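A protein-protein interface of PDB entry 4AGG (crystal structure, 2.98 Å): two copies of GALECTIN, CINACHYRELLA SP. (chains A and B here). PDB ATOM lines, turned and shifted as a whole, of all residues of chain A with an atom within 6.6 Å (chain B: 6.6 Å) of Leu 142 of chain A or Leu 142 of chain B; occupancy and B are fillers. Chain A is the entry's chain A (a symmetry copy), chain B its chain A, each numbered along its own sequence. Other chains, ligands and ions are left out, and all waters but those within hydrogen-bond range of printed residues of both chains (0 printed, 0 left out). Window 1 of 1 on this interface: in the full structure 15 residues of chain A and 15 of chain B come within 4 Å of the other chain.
Gln 5 of chain A touches Tyr 146 of chain B, and with the chains exchanged Tyr 146 of chain A touches Gln 5 of chain B.
Leu 139 of chain A touches Tyr 146 of chain B, and with the chains exchanged Tyr 146 of chain A touches Leu 139 of chain B.
Ser 143 of chain A touches its own counterpart, Ser 143 of chain B.
Of the 20 pairs that touch across the chains among the printed residues, 20 have their exchanged pair printed and touching as well.
Printed residues of chain B that touch a printed residue of chain A: Gln 5, Ser 6, Leu 139, Glu 140, Ser 141, Leu 142, Ser 143, Ala 144, Tyr 145 and Tyr 146.
Hydrophobic or aromatic side chains of chain B within 4 Å of the printed part of chain A: Leu 139, Leu 142 and Tyr 146.
Of the 18 printed residues of chain A, 10 touch a printed residue of chain B.
Printed residues of chain A that touch a printed residue of chain B: Gln 5, Ser 6, Leu 139, Glu 140, Ser 141, Leu 142, Ser 143, Ala 144, Tyr 145 and Tyr 146.
Hydrophobic or aromatic side chains of chain A within 4 Å of the printed part of chain B: Leu 139, Leu 142 and Tyr 146.
Along chain A the printed residues that touch a printed residue of chain B span positions 5 to 146.
Among the printed residues, no Asp or Glu carboxylate lies within 4 Å of a Lys or Arg side-chain nitrogen of the other chain.
O of Ser 141 of chain A sits at hydrogen-bond distance from N of Val 20 of chain A.
The backbone carbonyl oxygen (O) of Val 20 of chain B sits at hydrogen-bond distance from the backbone NH (N) of Glu 140 of chain B (2.7 Å).
The backbone carbonyl oxygen (O) of Gln 5 of chain A sits at hydrogen-bond distance from the backbone NH (N) of Tyr 126 of chain A, 2.7 Å away.
The backbone carbonyl oxygen (O) of Ser 141 of chain B lies within hydrogen-bond range of the backbone NH (N) of Val 20 of chain B, at 3.0 Å.
Printed residues of chain B within 4 Å of Ser 6 of chain A: Tyr 146.
Val 20 of chain A touches none of the printed residues of chain B.
Leu 142 of chain A touches just these residues of chain B: Leu 142 (3.7 Å), Ser 143 (3.2 Å), Ala 144 (3.0 Å) and Tyr 146 (3.9 Å).
Of the printed residues of chain B, Ser 143 of chain A touches Leu 142 and Ser 143.
Printed residues of chain B within 4 Å of Tyr 146 of chain A: Gln 5, Ser 6, Leu 139, Glu 140 and Leu 142.
Leu 142 of chain B touches four residues of chain A.
Of the printed residues of chain A, Ala 144 of chain B touches Ser 141 (3.3 Å) and Leu 142 (3.0 Å).
The nearest residue of chain B that does not touch Leu 142 of chain A is Tyr 145 of chain B (5.2 Å).
The backbone carbonyl oxygen (O) of Leu 142 of chain B sits at hydrogen-bond distance from the backbone NH (N) of Ala 144 of chain A (3.0 Å).
O of Glu 140 of chain B is in hydrogen-bond range of N of Tyr 146 of chain A (3.1 Å).
The backbone carbonyl oxygen (O) of Leu 142 of chain A lies within hydrogen-bond range of the backbone NH (N) of Ala 144 of chain B, 3.0 Å away.
N of Tyr 146 of chain B sits at hydrogen-bond distance from O of Glu 140 of chain A.
The side-chain hydroxyl (OG) of Ser 143 of chain B lies within hydrogen-bond range of the side-chain hydroxyl (OG) of Ser 143 of chain A.
Among the printed residues, merely in contact across the chains: Leu 142 of chain A with Ser 143 of chain B (3.2 Å), Ser 143 of chain A with Leu 142 of chain B (3.2 Å), Ala 144 of chain A with Ser 141 of chain B (3.3 Å), Ser 141 of chain A with Ala 144 of chain B (3.3 Å), Gln 5 of chain A with Tyr 146 of chain B (3.4 Å), Tyr 146 of chain A with Gln 5 of chain B (3.4 Å), Tyr 145 of chain A with Glu 140 of chain B (3.5 Å), Glu 140 of chain A with Tyr 145 of chain B (3.5 Å), Leu 139 of chain A with Tyr 146 of chain B (3.6 Å), Tyr 146 of chain A with Leu 139 of chain B (3.6 Å), Ser 6 of chain A with Tyr 146 of chain B (3.6 Å), Tyr 146 of chain A with Ser 6 of chain B (3.6 Å), Leu 142 of chain A with Leu 142 of chain B (3.7 Å), Leu 142 of chain A with Tyr 146 of chain B (3.9 Å) and Tyr 146 of chain A with Leu 142 of chain B (3.9 Å).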
ATOM      1  N   GLN A   5      -6.604 -11.765 -31.081  1.00  0.00           N
ATOM      2  CA  GLN A   5      -5.140 -11.747 -31.024  1.00  0.00           C
ATOM      3  C   GLN A   5      -4.478 -13.034 -31.528  1.00  0.00           C
ATOM      4  O   GLN A   5      -5.057 -14.133 -31.489  1.00  0.00           O
ATOM      5  CB  GLN A   5      -4.711 -11.416 -29.606  1.00  0.00           C
ATOM      6  CG  GLN A   5      -5.044  -9.988 -29.229  1.00  0.00           C
ATOM      7  CD  GLN A   5      -3.976  -9.057 -29.715  1.00  0.00           C
ATOM      8  OE1 GLN A   5      -3.053  -9.468 -30.424  1.00  0.00           O
ATOM      9  NE2 GLN A   5      -4.060  -7.811 -29.307  1.00  0.00           N
ATOM     10  N   SER A   6      -3.266 -12.902 -32.030  1.00  0.00           N
ATOM     11  CA  SER A   6      -2.579 -14.080 -32.530  1.00  0.00           C
ATOM     12  C   SER A   6      -1.051 -13.962 -32.520  1.00  0.00           C
ATOM     13  O   SER A   6      -0.466 -12.896 -32.212  1.00  0.00           O
ATOM     14  CB  SER A   6      -3.058 -14.399 -33.936  1.00  0.00           C
ATOM     15  OG  SER A   6      -2.742 -13.318 -34.797  1.00  0.00           O
ATOM     16  N   ILE A   7      -0.430 -15.101 -32.823  1.00  0.00           N
ATOM     17  CA  ILE A   7       1.005 -15.234 -32.969  1.00  0.00           C
ATOM     18  C   ILE A   7       1.231 -16.044 -34.222  1.00  0.00           C
ATOM     19  O   ILE A   7       0.475 -16.990 -34.502  1.00  0.00           O
ATOM     20  CB  ILE A   7       1.683 -15.960 -31.775  1.00  0.00           C
ATOM     21  CG1 ILE A   7       1.037 -17.297 -31.462  1.00  0.00           C
ATOM     22  CG2 ILE A   7       1.643 -15.133 -30.501  1.00  0.00           C
ATOM     23  CD1 ILE A   7       1.721 -18.024 -30.319  1.00  0.00           C
ATOM     24  N   GLY A  18      -0.210 -22.557 -26.404  1.00  0.00           N
ATOM     25  CA  GLY A  18      -0.835 -22.321 -25.169  1.00  0.00           C
ATOM     26  C   GLY A  18      -1.366 -20.933 -25.211  1.00  0.00           C
ATOM     27  O   GLY A  18      -0.729 -20.030 -25.773  1.00  0.00           O
ATOM     28  N   VAL A  19      -2.561 -20.820 -24.617  1.00  0.00           N
ATOM     29  CA  VAL A  19      -3.214 -19.577 -24.228  1.00  0.00           C
ATOM     30  C   VAL A  19      -3.608 -19.647 -22.770  1.00  0.00           C
ATOM     31  O   VAL A  19      -3.875 -20.726 -22.227  1.00  0.00           O
ATOM     32  CB  VAL A  19      -4.528 -19.350 -25.007  1.00  0.00           C
ATOM     33  CG1 VAL A  19      -5.522 -20.487 -24.767  1.00  0.00           C
ATOM     34  CG2 VAL A  19      -5.163 -18.018 -24.631  1.00  0.00           C
ATOM     35  N   VAL A  20      -3.644 -18.468 -22.165  1.00  0.00           N
ATOM     36  CA  VAL A  20      -4.152 -18.245 -20.840  1.00  0.00           C
ATOM     37  C   VAL A  20      -5.078 -17.029 -20.880  1.00  0.00           C
ATOM     38  O   VAL A  20      -4.671 -15.954 -21.341  1.00  0.00           O
ATOM     39  CB  VAL A  20      -3.000 -17.965 -19.879  1.00  0.00           C
ATOM     40  CG1 VAL A  20      -3.515 -17.392 -18.552  1.00  0.00           C
ATOM     41  CG2 VAL A  20      -2.249 -19.247 -19.671  1.00  0.00           C
ATOM     42  N   LEU A  31     -10.270 -20.920 -30.486  1.00  0.00           N
ATOM     43  CA  LEU A  31      -8.860 -21.025 -30.794  1.00  0.00           C
ATOM     44  C   LEU A  31      -8.700 -21.642 -32.131  1.00  0.00           C
ATOM     45  O   LEU A  31      -9.122 -22.789 -32.358  1.00  0.00           O
ATOM     46  CB  LEU A  31      -8.137 -21.897 -29.782  1.00  0.00           C
ATOM     47  CG  LEU A  31      -8.346 -21.441 -28.348  1.00  0.00           C
ATOM     48  CD1 LEU A  31      -7.700 -22.392 -27.356  1.00  0.00           C
ATOM     49  CD2 LEU A  31      -7.834 -20.016 -28.188  1.00  0.00           C
ATOM     50  N   PHE A 124      -1.683 -19.115 -34.493  1.00  0.00           N
ATOM     51  CA  PHE A 124      -2.414 -19.472 -33.290  1.00  0.00           C
ATOM     52  C   PHE A 124      -3.215 -18.268 -32.897  1.00  0.00           C
ATOM     53  O   PHE A 124      -2.650 -17.233 -32.509  1.00  0.00           O
ATOM     54  CB  PHE A 124      -1.463 -19.821 -32.156  1.00  0.00           C
ATOM     55  CG  PHE A 124      -2.148 -20.334 -30.915  1.00  0.00           C
ATOM     56  CD1 PHE A 124      -2.960 -21.449 -30.962  1.00  0.00           C
ATOM     57  CD2 PHE A 124      -1.951 -19.717 -29.700  1.00  0.00           C
ATOM     58  CE1 PHE A 124      -3.574 -21.930 -29.820  1.00  0.00           C
ATOM     59  CE2 PHE A 124      -2.561 -20.189 -28.549  1.00  0.00           C
ATOM     60  CZ  PHE A 124      -3.372 -21.301 -28.604  1.00  0.00           C
ATOM     61  N   GLN A 125      -4.532 -18.414 -32.997  1.00  0.00           N
ATOM     62  CA  GLN A 125      -5.414 -17.276 -32.855  1.00  0.00           C
ATOM     63  C   GLN A 125      -6.392 -17.415 -31.724  1.00  0.00           C
ATOM     64  O   GLN A 125      -6.933 -18.504 -31.496  1.00  0.00           O
ATOM     65  CB  GLN A 125      -6.170 -17.047 -34.143  1.00  0.00           C
ATOM     66  CG  GLN A 125      -6.949 -15.758 -34.139  1.00  0.00           C
ATOM     67  CD  GLN A 125      -7.104 -15.206 -35.533  1.00  0.00           C
ATOM     68  OE1 GLN A 125      -7.781 -15.790 -36.375  1.00  0.00           O
ATOM     69  NE2 GLN A 125      -6.469 -14.071 -35.787  1.00  0.00           N
ATOM     70  N   TYR A 126      -6.615 -16.283 -31.047  1.00  0.00           N
ATOM     71  CA  TYR A 126      -7.588 -16.126 -29.976  1.00  0.00           C
ATOM     72  C   TYR A 126      -8.682 -15.233 -30.496  1.00  0.00           C
ATOM     73  O   TYR A 126      -8.387 -14.145 -31.005  1.00  0.00           O
ATOM     74  CB  TYR A 126      -6.919 -15.435 -28.783  1.00  0.00           C
ATOM     75  CG  TYR A 126      -7.851 -14.884 -27.676  1.00  0.00           C
ATOM     76  CD1 TYR A 126      -8.312 -15.711 -26.635  1.00  0.00           C
ATOM     77  CD2 TYR A 126      -8.242 -13.530 -27.650  1.00  0.00           C
ATOM     78  CE1 TYR A 126      -9.145 -15.221 -25.632  1.00  0.00           C
ATOM     79  CE2 TYR A 126      -9.074 -13.051 -26.648  1.00  0.00           C
ATOM     80  CZ  TYR A 126      -9.522 -13.903 -25.642  1.00  0.00           C
ATOM     81  OH  TYR A 126     -10.341 -13.439 -24.634  1.00  0.00           O
ATOM     82  N   LEU A 139      -7.839 -11.691 -22.401  1.00  0.00           N
ATOM     83  CA  LEU A 139      -6.720 -12.589 -22.726  1.00  0.00           C
ATOM     84  C   LEU A 139      -5.462 -12.229 -21.989  1.00  0.00           C
ATOM     85  O   LEU A 139      -5.158 -11.039 -21.860  1.00  0.00           O
ATOM     86  CB  LEU A 139      -6.417 -12.497 -24.211  1.00  0.00           C
ATOM     87  CG  LEU A 139      -5.064 -12.977 -24.729  1.00  0.00           C
ATOM     88  CD1 LEU A 139      -5.049 -14.501 -24.808  1.00  0.00           C
ATOM     89  CD2 LEU A 139      -4.833 -12.315 -26.080  1.00  0.00           C
ATOM     90  N   GLU A 140      -4.705 -13.234 -21.554  1.00  0.00           N
ATOM     91  CA  GLU A 140      -3.467 -12.979 -20.778  1.00  0.00           C
ATOM     92  C   GLU A 140      -2.138 -13.281 -21.471  1.00  0.00           C
ATOM     93  O   GLU A 140      -1.239 -12.445 -21.460  1.00  0.00           O
ATOM     94  CB  GLU A 140      -3.504 -13.751 -19.477  1.00  0.00           C
ATOM     95  CG  GLU A 140      -4.796 -13.567 -18.719  1.00  0.00           C
ATOM     96  CD  GLU A 140      -4.561 -13.392 -17.229  1.00  0.00           C
ATOM     97  OE1 GLU A 140      -3.563 -13.995 -16.722  1.00  0.00           O
ATOM     98  OE2 GLU A 140      -5.375 -12.652 -16.588  1.00  0.00           O
ATOM     99  N   SER A 141      -2.029 -14.485 -22.040  1.00  0.00           N
ATOM    100  CA  SER A 141      -0.789 -14.980 -22.627  1.00  0.00           C
ATOM    101  C   SER A 141      -1.046 -15.906 -23.839  1.00  0.00           C
ATOM    102  O   SER A 141      -2.031 -16.653 -23.887  1.00  0.00           O
ATOM    103  CB  SER A 141       0.037 -15.742 -21.578  1.00  0.00           C
ATOM    104  OG  SER A 141      -0.007 -17.156 -21.814  1.00  0.00           O
ATOM    105  N   LEU A 142      -0.106 -15.868 -24.785  1.00  0.00           N
ATOM    106  CA  LEU A 142      -0.112 -16.677 -26.007  1.00  0.00           C
ATOM    107  C   LEU A 142       1.271 -17.266 -26.150  1.00  0.00           C
ATOM    108  O   LEU A 142       2.276 -16.559 -25.988  1.00  0.00           O
ATOM    109  CB  LEU A 142      -0.459 -15.811 -27.207  1.00  0.00           C
ATOM    110  CG  LEU A 142      -1.967 -15.602 -27.298  1.00  0.00           C
ATOM    111  CD1 LEU A 142      -2.401 -14.914 -28.582  1.00  0.00           C
ATOM    112  CD2 LEU A 142      -2.630 -16.965 -27.204  1.00  0.00           C
ATOM    113  N   SER A 143       1.345 -18.562 -26.404  1.00  0.00           N
ATOM    114  CA  SER A 143       2.592 -19.202 -26.144  1.00  0.00           C
ATOM    115  C   SER A 143       2.792 -20.373 -27.011  1.00  0.00           C
ATOM    116  O   SER A 143       1.905 -21.210 -27.155  1.00  0.00           O
ATOM    117  CB  SER A 143       2.685 -19.644 -24.682  1.00  0.00           C
ATOM    118  OG  SER A 143       2.726 -18.521 -23.825  1.00  0.00           O
ATOM    119  N   ALA A 144       3.989 -20.418 -27.578  1.00  0.00           N
ATOM    120  CA  ALA A 144       4.438 -21.569 -28.289  1.00  0.00           C
ATOM    121  C   ALA A 144       5.417 -22.283 -27.436  1.00  0.00           C
ATOM    122  O   ALA A 144       6.181 -21.667 -26.678  1.00  0.00           O
ATOM    123  CB  ALA A 144       5.118 -21.160 -29.545  1.00  0.00           C
ATOM    124  N   TYR A 145       5.418 -23.595 -27.608  1.00  0.00           N
ATOM    125  CA  TYR A 145       6.227 -24.472 -26.826  1.00  0.00           C
ATOM    126  C   TYR A 145       6.921 -25.360 -27.774  1.00  0.00           C
ATOM    127  O   TYR A 145       6.309 -25.883 -28.715  1.00  0.00           O
ATOM    128  CB  TYR A 145       5.346 -25.311 -25.961  1.00  0.00           C
ATOM    129  CG  TYR A 145       4.611 -24.506 -24.928  1.00  0.00           C
ATOM    130  CD1 TYR A 145       3.376 -23.877 -25.223  1.00  0.00           C
ATOM    131  CD2 TYR A 145       5.153 -24.370 -23.642  1.00  0.00           C
ATOM    132  CE1 TYR A 145       2.728 -23.146 -24.247  1.00  0.00           C
ATOM    133  CE2 TYR A 145       4.515 -23.636 -22.671  1.00  0.00           C
ATOM    134  CZ  TYR A 145       3.320 -23.035 -22.972  1.00  0.00           C
ATOM    135  OH  TYR A 145       2.747 -22.342 -21.966  1.00  0.00           O
ATOM    136  N   TYR A 146       8.200 -25.564 -27.479  1.00  0.00           N
ATOM    137  CA  TYR A 146       9.163 -26.184 -28.390  1.00  0.00           C
ATOM    138  C   TYR A 146       9.865 -27.454 -27.854  1.00  0.00           C
ATOM    139  O   TYR A 146      10.121 -28.439 -28.574  1.00  0.00           O
ATOM    140  CB  TYR A 146      10.206 -25.132 -28.739  1.00  0.00           C
ATOM    141  CG  TYR A 146       9.637 -24.003 -29.529  1.00  0.00           C
ATOM    142  CD1 TYR A 146       9.438 -24.136 -30.898  1.00  0.00           C
ATOM    143  CD2 TYR A 146       9.277 -22.798 -28.916  1.00  0.00           C
ATOM    144  CE1 TYR A 146       8.924 -23.099 -31.638  1.00  0.00           C
ATOM    145  CE2 TYR A 146       8.762 -21.746 -29.663  1.00  0.00           C
ATOM    146  CZ  TYR A 146       8.589 -21.915 -31.015  1.00  0.00           C
ATOM    147  OH  TYR A 146       8.084 -20.911 -31.792  1.00  0.00           O
ATOM    148  OXT TYR A 146      10.237 -27.510 -26.678  1.00  0.00           O
ATOM    149  N   GLN B   5      14.338 -19.412 -33.577  1.00  0.00           N
ATOM    150  CA  GLN B   5      12.876 -19.468 -33.506  1.00  0.00           C
ATOM    151  C   GLN B   5      12.211 -18.116 -33.220  1.00  0.00           C
ATOM    152  O   GLN B   5      12.799 -17.209 -32.607  1.00  0.00           O
ATOM    153  CB  GLN B   5      12.477 -20.514 -32.481  1.00  0.00           C
ATOM    154  CG  GLN B   5      12.809 -21.918 -32.942  1.00  0.00           C
ATOM    155  CD  GLN B   5      11.725 -22.446 -33.830  1.00  0.00           C
ATOM    156  OE1 GLN B   5      10.788 -21.723 -34.184  1.00  0.00           O
ATOM    157  NE2 GLN B   5      11.809 -23.714 -34.161  1.00  0.00           N
ATOM    158  N   SER B   6      10.987 -17.964 -33.687  1.00  0.00           N
ATOM    159  CA  SER B   6      10.298 -16.708 -33.456  1.00  0.00           C
ATOM    160  C   SER B   6       8.769 -16.822 -33.478  1.00  0.00           C
ATOM    161  O   SER B   6       8.184 -17.890 -33.780  1.00  0.00           O
ATOM    162  CB  SER B   6      10.748 -15.677 -34.478  1.00  0.00           C
ATOM    163  OG  SER B   6      10.405 -16.125 -35.779  1.00  0.00           O
ATOM    164  N   ILE B   7       8.150 -15.704 -33.104  1.00  0.00           N
ATOM    165  CA  ILE B   7       6.713 -15.523 -33.123  1.00  0.00           C
ATOM    166  C   ILE B   7       6.463 -14.166 -33.735  1.00  0.00           C
ATOM    167  O   ILE B   7       7.219 -13.213 -33.478  1.00  0.00           O
ATOM    168  CB  ILE B   7       6.066 -15.561 -31.712  1.00  0.00           C
ATOM    169  CG1 ILE B   7       6.728 -14.599 -30.741  1.00  0.00           C
ATOM    170  CG2 ILE B   7       6.129 -16.944 -31.086  1.00  0.00           C
ATOM    171  CD1 ILE B   7       6.074 -14.609 -29.371  1.00  0.00           C
ATOM    172  N   GLY B  18       8.122 -12.893 -23.673  1.00  0.00           N
ATOM    173  CA  GLY B  18       8.773 -13.754 -22.775  1.00  0.00           C
ATOM    174  C   GLY B  18       9.293 -14.897 -23.572  1.00  0.00           C
ATOM    175  O   GLY B  18       8.638 -15.358 -24.518  1.00  0.00           O
ATOM    176  N   VAL B  19      10.501 -15.304 -23.160  1.00  0.00           N
ATOM    177  CA  VAL B  19      11.154 -16.557 -23.517  1.00  0.00           C
ATOM    178  C   VAL B  19      11.582 -17.283 -22.261  1.00  0.00           C
ATOM    179  O   VAL B  19      11.867 -16.665 -21.228  1.00  0.00           O
ATOM    180  CB  VAL B  19      12.449 -16.319 -24.325  1.00  0.00           C
ATOM    181  CG1 VAL B  19      13.456 -15.485 -23.532  1.00  0.00           C
ATOM    182  CG2 VAL B  19      13.084 -17.639 -24.741  1.00  0.00           C
ATOM    183  N   VAL B  20      11.623 -18.601 -22.390  1.00  0.00           N
ATOM    184  CA  VAL B  20      12.159 -19.501 -21.406  1.00  0.00           C
ATOM    185  C   VAL B  20      13.076 -20.496 -22.116  1.00  0.00           C
ATOM    186  O   VAL B  20      12.651 -21.156 -23.076  1.00  0.00           O
ATOM    187  CB  VAL B  20      11.027 -20.263 -20.723  1.00  0.00           C
ATOM    188  CG1 VAL B  20      11.568 -21.457 -19.927  1.00  0.00           C
ATOM    189  CG2 VAL B  20      10.289 -19.300 -19.839  1.00  0.00           C
ATOM    190  N   LEU B  31      18.077 -12.002 -28.217  1.00  0.00           N
ATOM    191  CA  LEU B  31      16.661 -11.757 -28.387  1.00  0.00           C
ATOM    192  C   LEU B  31      16.476 -10.517 -29.176  1.00  0.00           C
ATOM    193  O   LEU B  31      16.900  -9.426 -28.757  1.00  0.00           O
ATOM    194  CB  LEU B  31      15.967 -11.574 -27.050  1.00  0.00           C
ATOM    195  CG  LEU B  31      16.205 -12.730 -26.093  1.00  0.00           C
ATOM    196  CD1 LEU B  31      15.587 -12.469 -24.731  1.00  0.00           C
ATOM    197  CD2 LEU B  31      15.687 -14.019 -26.716  1.00  0.00           C
ATOM    198  N   PHE B 124       9.391 -11.415 -32.372  1.00  0.00           N
ATOM    199  CA  PHE B 124      10.151 -11.760 -31.182  1.00  0.00           C
ATOM    200  C   PHE B 124      10.953 -12.979 -31.519  1.00  0.00           C
ATOM    201  O   PHE B 124      10.390 -14.065 -31.739  1.00  0.00           O
ATOM    202  CB  PHE B 124       9.227 -12.084 -30.019  1.00  0.00           C
ATOM    203  CG  PHE B 124       9.944 -12.318 -28.713  1.00  0.00           C
ATOM    204  CD1 PHE B 124      10.762 -11.348 -28.169  1.00  0.00           C
ATOM    205  CD2 PHE B 124       9.770 -13.493 -28.018  1.00  0.00           C
ATOM    206  CE1 PHE B 124      11.404 -11.555 -26.961  1.00  0.00           C
ATOM    207  CE2 PHE B 124      10.408 -13.714 -26.809  1.00  0.00           C
ATOM    208  CZ  PHE B 124      11.226 -12.742 -26.274  1.00  0.00           C
ATOM    209  N   GLN B 125      12.268 -12.794 -31.554  1.00  0.00           N
ATOM    210  CA  GLN B 125      13.146 -13.824 -32.068  1.00  0.00           C
ATOM    211  C   GLN B 125      14.150 -14.310 -31.063  1.00  0.00           C
ATOM    212  O   GLN B 125      14.703 -13.513 -30.296  1.00  0.00           O
ATOM    213  CB  GLN B 125      13.871 -13.316 -33.292  1.00  0.00           C
ATOM    214  CG  GLN B 125      14.641 -14.398 -34.002  1.00  0.00           C
ATOM    215  CD  GLN B 125      14.762 -14.109 -35.477  1.00  0.00           C
ATOM    216  OE1 GLN B 125      15.424 -13.159 -35.885  1.00  0.00           O
ATOM    217  NE2 GLN B 125      14.113 -14.932 -36.289  1.00  0.00           N
ATOM    218  N   TYR B 126      14.380 -15.627 -31.110  1.00  0.00           N
ATOM    219  CA  TYR B 126      15.375 -16.331 -30.314  1.00  0.00           C
ATOM    220  C   TYR B 126      16.452 -16.795 -31.259  1.00  0.00           C
ATOM    221  O   TYR B 126      16.139 -17.438 -32.268  1.00  0.00           O
ATOM    222  CB  TYR B 126      14.729 -17.561 -29.669  1.00  0.00           C
ATOM    223  CG  TYR B 126      15.682 -18.616 -29.056  1.00  0.00           C
ATOM    224  CD1 TYR B 126      16.171 -18.479 -27.744  1.00  0.00           C
ATOM    225  CD2 TYR B 126      16.064 -19.767 -29.773  1.00  0.00           C
ATOM    226  CE1 TYR B 126      17.024 -19.427 -27.183  1.00  0.00           C
ATOM    227  CE2 TYR B 126      16.916 -20.706 -29.207  1.00  0.00           C
ATOM    228  CZ  TYR B 126      17.392 -20.529 -27.910  1.00  0.00           C
ATOM    229  OH  TYR B 126      18.230 -21.458 -27.331  1.00  0.00           O
ATOM    230  N   LEU B 139      15.767 -24.151 -26.340  1.00  0.00           N
ATOM    231  CA  LEU B 139      14.647 -23.227 -26.103  1.00  0.00           C
ATOM    232  C   LEU B 139      13.404 -23.936 -25.650  1.00  0.00           C
ATOM    233  O   LEU B 139      13.095 -25.010 -26.176  1.00  0.00           O
ATOM    234  CB  LEU B 139      14.310 -22.505 -27.395  1.00  0.00           C
ATOM    235  CG  LEU B 139      12.949 -21.830 -27.543  1.00  0.00           C
ATOM    236  CD1 LEU B 139      12.942 -20.505 -26.786  1.00  0.00           C
ATOM    237  CD2 LEU B 139      12.684 -21.659 -29.032  1.00  0.00           C
ATOM    238  N   GLU B 140      12.662 -23.330 -24.724  1.00  0.00           N
ATOM    239  CA  GLU B 140      11.441 -23.971 -24.180  1.00  0.00           C
ATOM    240  C   GLU B 140      10.099 -23.352 -24.571  1.00  0.00           C
ATOM    241  O   GLU B 140       9.194 -24.068 -24.993  1.00  0.00           O
ATOM    242  CB  GLU B 140      11.512 -24.023 -22.670  1.00  0.00           C
ATOM    243  CG  GLU B 140      12.820 -24.579 -22.161  1.00  0.00           C
ATOM    244  CD  GLU B 140      12.617 -25.532 -20.995  1.00  0.00           C
ATOM    245  OE1 GLU B 140      11.634 -25.304 -20.221  1.00  0.00           O
ATOM    246  OE2 GLU B 140      13.440 -26.495 -20.874  1.00  0.00           O
ATOM    247  N   SER B 141       9.985 -22.032 -24.398  1.00  0.00           N
ATOM    248  CA  SER B 141       8.735 -21.306 -24.597  1.00  0.00           C
ATOM    249  C   SER B 141       8.971 -19.871 -25.122  1.00  0.00           C
ATOM    250  O   SER B 141       9.960 -19.210 -24.782  1.00  0.00           O
ATOM    251  CB  SER B 141       7.938 -21.236 -23.284  1.00  0.00           C
ATOM    252  OG  SER B 141       7.986 -19.919 -22.721  1.00  0.00           O
ATOM    253  N   LEU B 142       8.010 -19.399 -25.919  1.00  0.00           N
ATOM    254  CA  LEU B 142       7.994 -18.058 -26.510  1.00  0.00           C
ATOM    255  C   LEU B 142       6.612 -17.494 -26.281  1.00  0.00           C
ATOM    256  O   LEU B 142       5.607 -18.183 -26.504  1.00  0.00           O
ATOM    257  CB  LEU B 142       8.309 -18.137 -27.995  1.00  0.00           C
ATOM    258  CG  LEU B 142       9.813 -18.254 -28.219  1.00  0.00           C
ATOM    259  CD1 LEU B 142      10.214 -18.138 -29.680  1.00  0.00           C
ATOM    260  CD2 LEU B 142      10.486 -17.153 -27.419  1.00  0.00           C
ATOM    261  N   SER B 143       6.541 -16.266 -25.795  1.00  0.00           N
ATOM    262  CA  SER B 143       5.304 -15.877 -25.203  1.00  0.00           C
ATOM    263  C   SER B 143       5.093 -14.424 -25.295  1.00  0.00           C
ATOM    264  O   SER B 143       5.982 -13.636 -24.985  1.00  0.00           O
ATOM    265  CB  SER B 143       5.247 -16.294 -23.731  1.00  0.00           C
ATOM    266  OG  SER B 143       5.218 -17.702 -23.615  1.00  0.00           O
ATOM    267  N   ALA B 144       3.884 -14.088 -25.722  1.00  0.00           N
ATOM    268  CA  ALA B 144       3.427 -12.738 -25.689  1.00  0.00           C
ATOM    269  C   ALA B 144       2.471 -12.604 -24.564  1.00  0.00           C
ATOM    270  O   ALA B 144       1.720 -13.536 -24.241  1.00  0.00           O
ATOM    271  CB  ALA B 144       2.716 -12.409 -26.951  1.00  0.00           C
ATOM    272  N   TYR B 145       2.475 -11.406 -24.000  1.00  0.00           N
ATOM    273  CA  TYR B 145       1.689 -11.096 -22.851  1.00  0.00           C
ATOM    274  C   TYR B 145       0.981  -9.841 -23.154  1.00  0.00           C
ATOM    275  O   TYR B 145       1.575  -8.889 -23.677  1.00  0.00           O
ATOM    276  CB  TYR B 145       2.596 -10.850 -21.690  1.00  0.00           C
ATOM    277  CG  TYR B 145       3.348 -12.080 -21.271  1.00  0.00           C
ATOM    278  CD1 TYR B 145       4.571 -12.443 -21.887  1.00  0.00           C
ATOM    279  CD2 TYR B 145       2.834 -12.892 -20.250  1.00  0.00           C
ATOM    280  CE1 TYR B 145       5.237 -13.581 -21.474  1.00  0.00           C
ATOM    281  CE2 TYR B 145       3.488 -14.030 -19.844  1.00  0.00           C
ATOM    282  CZ  TYR B 145       4.672 -14.366 -20.448  1.00  0.00           C
ATOM    283  OH  TYR B 145       5.263 -15.489 -19.988  1.00  0.00           O
ATOM    284  N   TYR B 146      -0.290  -9.837 -22.767  1.00  0.00           N
ATOM    285  CA  TYR B 146      -1.269  -8.830 -23.177  1.00  0.00           C
ATOM    286  C   TYR B 146      -1.951  -8.055 -22.025  1.00  0.00           C
ATOM    287  O   TYR B 146      -2.217  -6.838 -22.093  1.00  0.00           O
ATOM    288  CB  TYR B 146      -2.327  -9.534 -24.016  1.00  0.00           C
ATOM    289  CG  TYR B 146      -1.783 -10.054 -25.303  1.00  0.00           C
ATOM    290  CD1 TYR B 146      -1.614  -9.202 -26.387  1.00  0.00           C
ATOM    291  CD2 TYR B 146      -1.417 -11.397 -25.445  1.00  0.00           C
ATOM    292  CE1 TYR B 146      -1.123  -9.672 -27.581  1.00  0.00           C
ATOM    293  CE2 TYR B 146      -0.926 -11.876 -26.653  1.00  0.00           C
ATOM    294  CZ  TYR B 146      -0.782 -11.002 -27.703  1.00  0.00           C
ATOM    295  OH  TYR B 146      -0.301 -11.426 -28.911  1.00  0.00           O
ATOM    296  OXT TYR B 146      -2.296  -8.644 -20.997  1.00  0.00           O
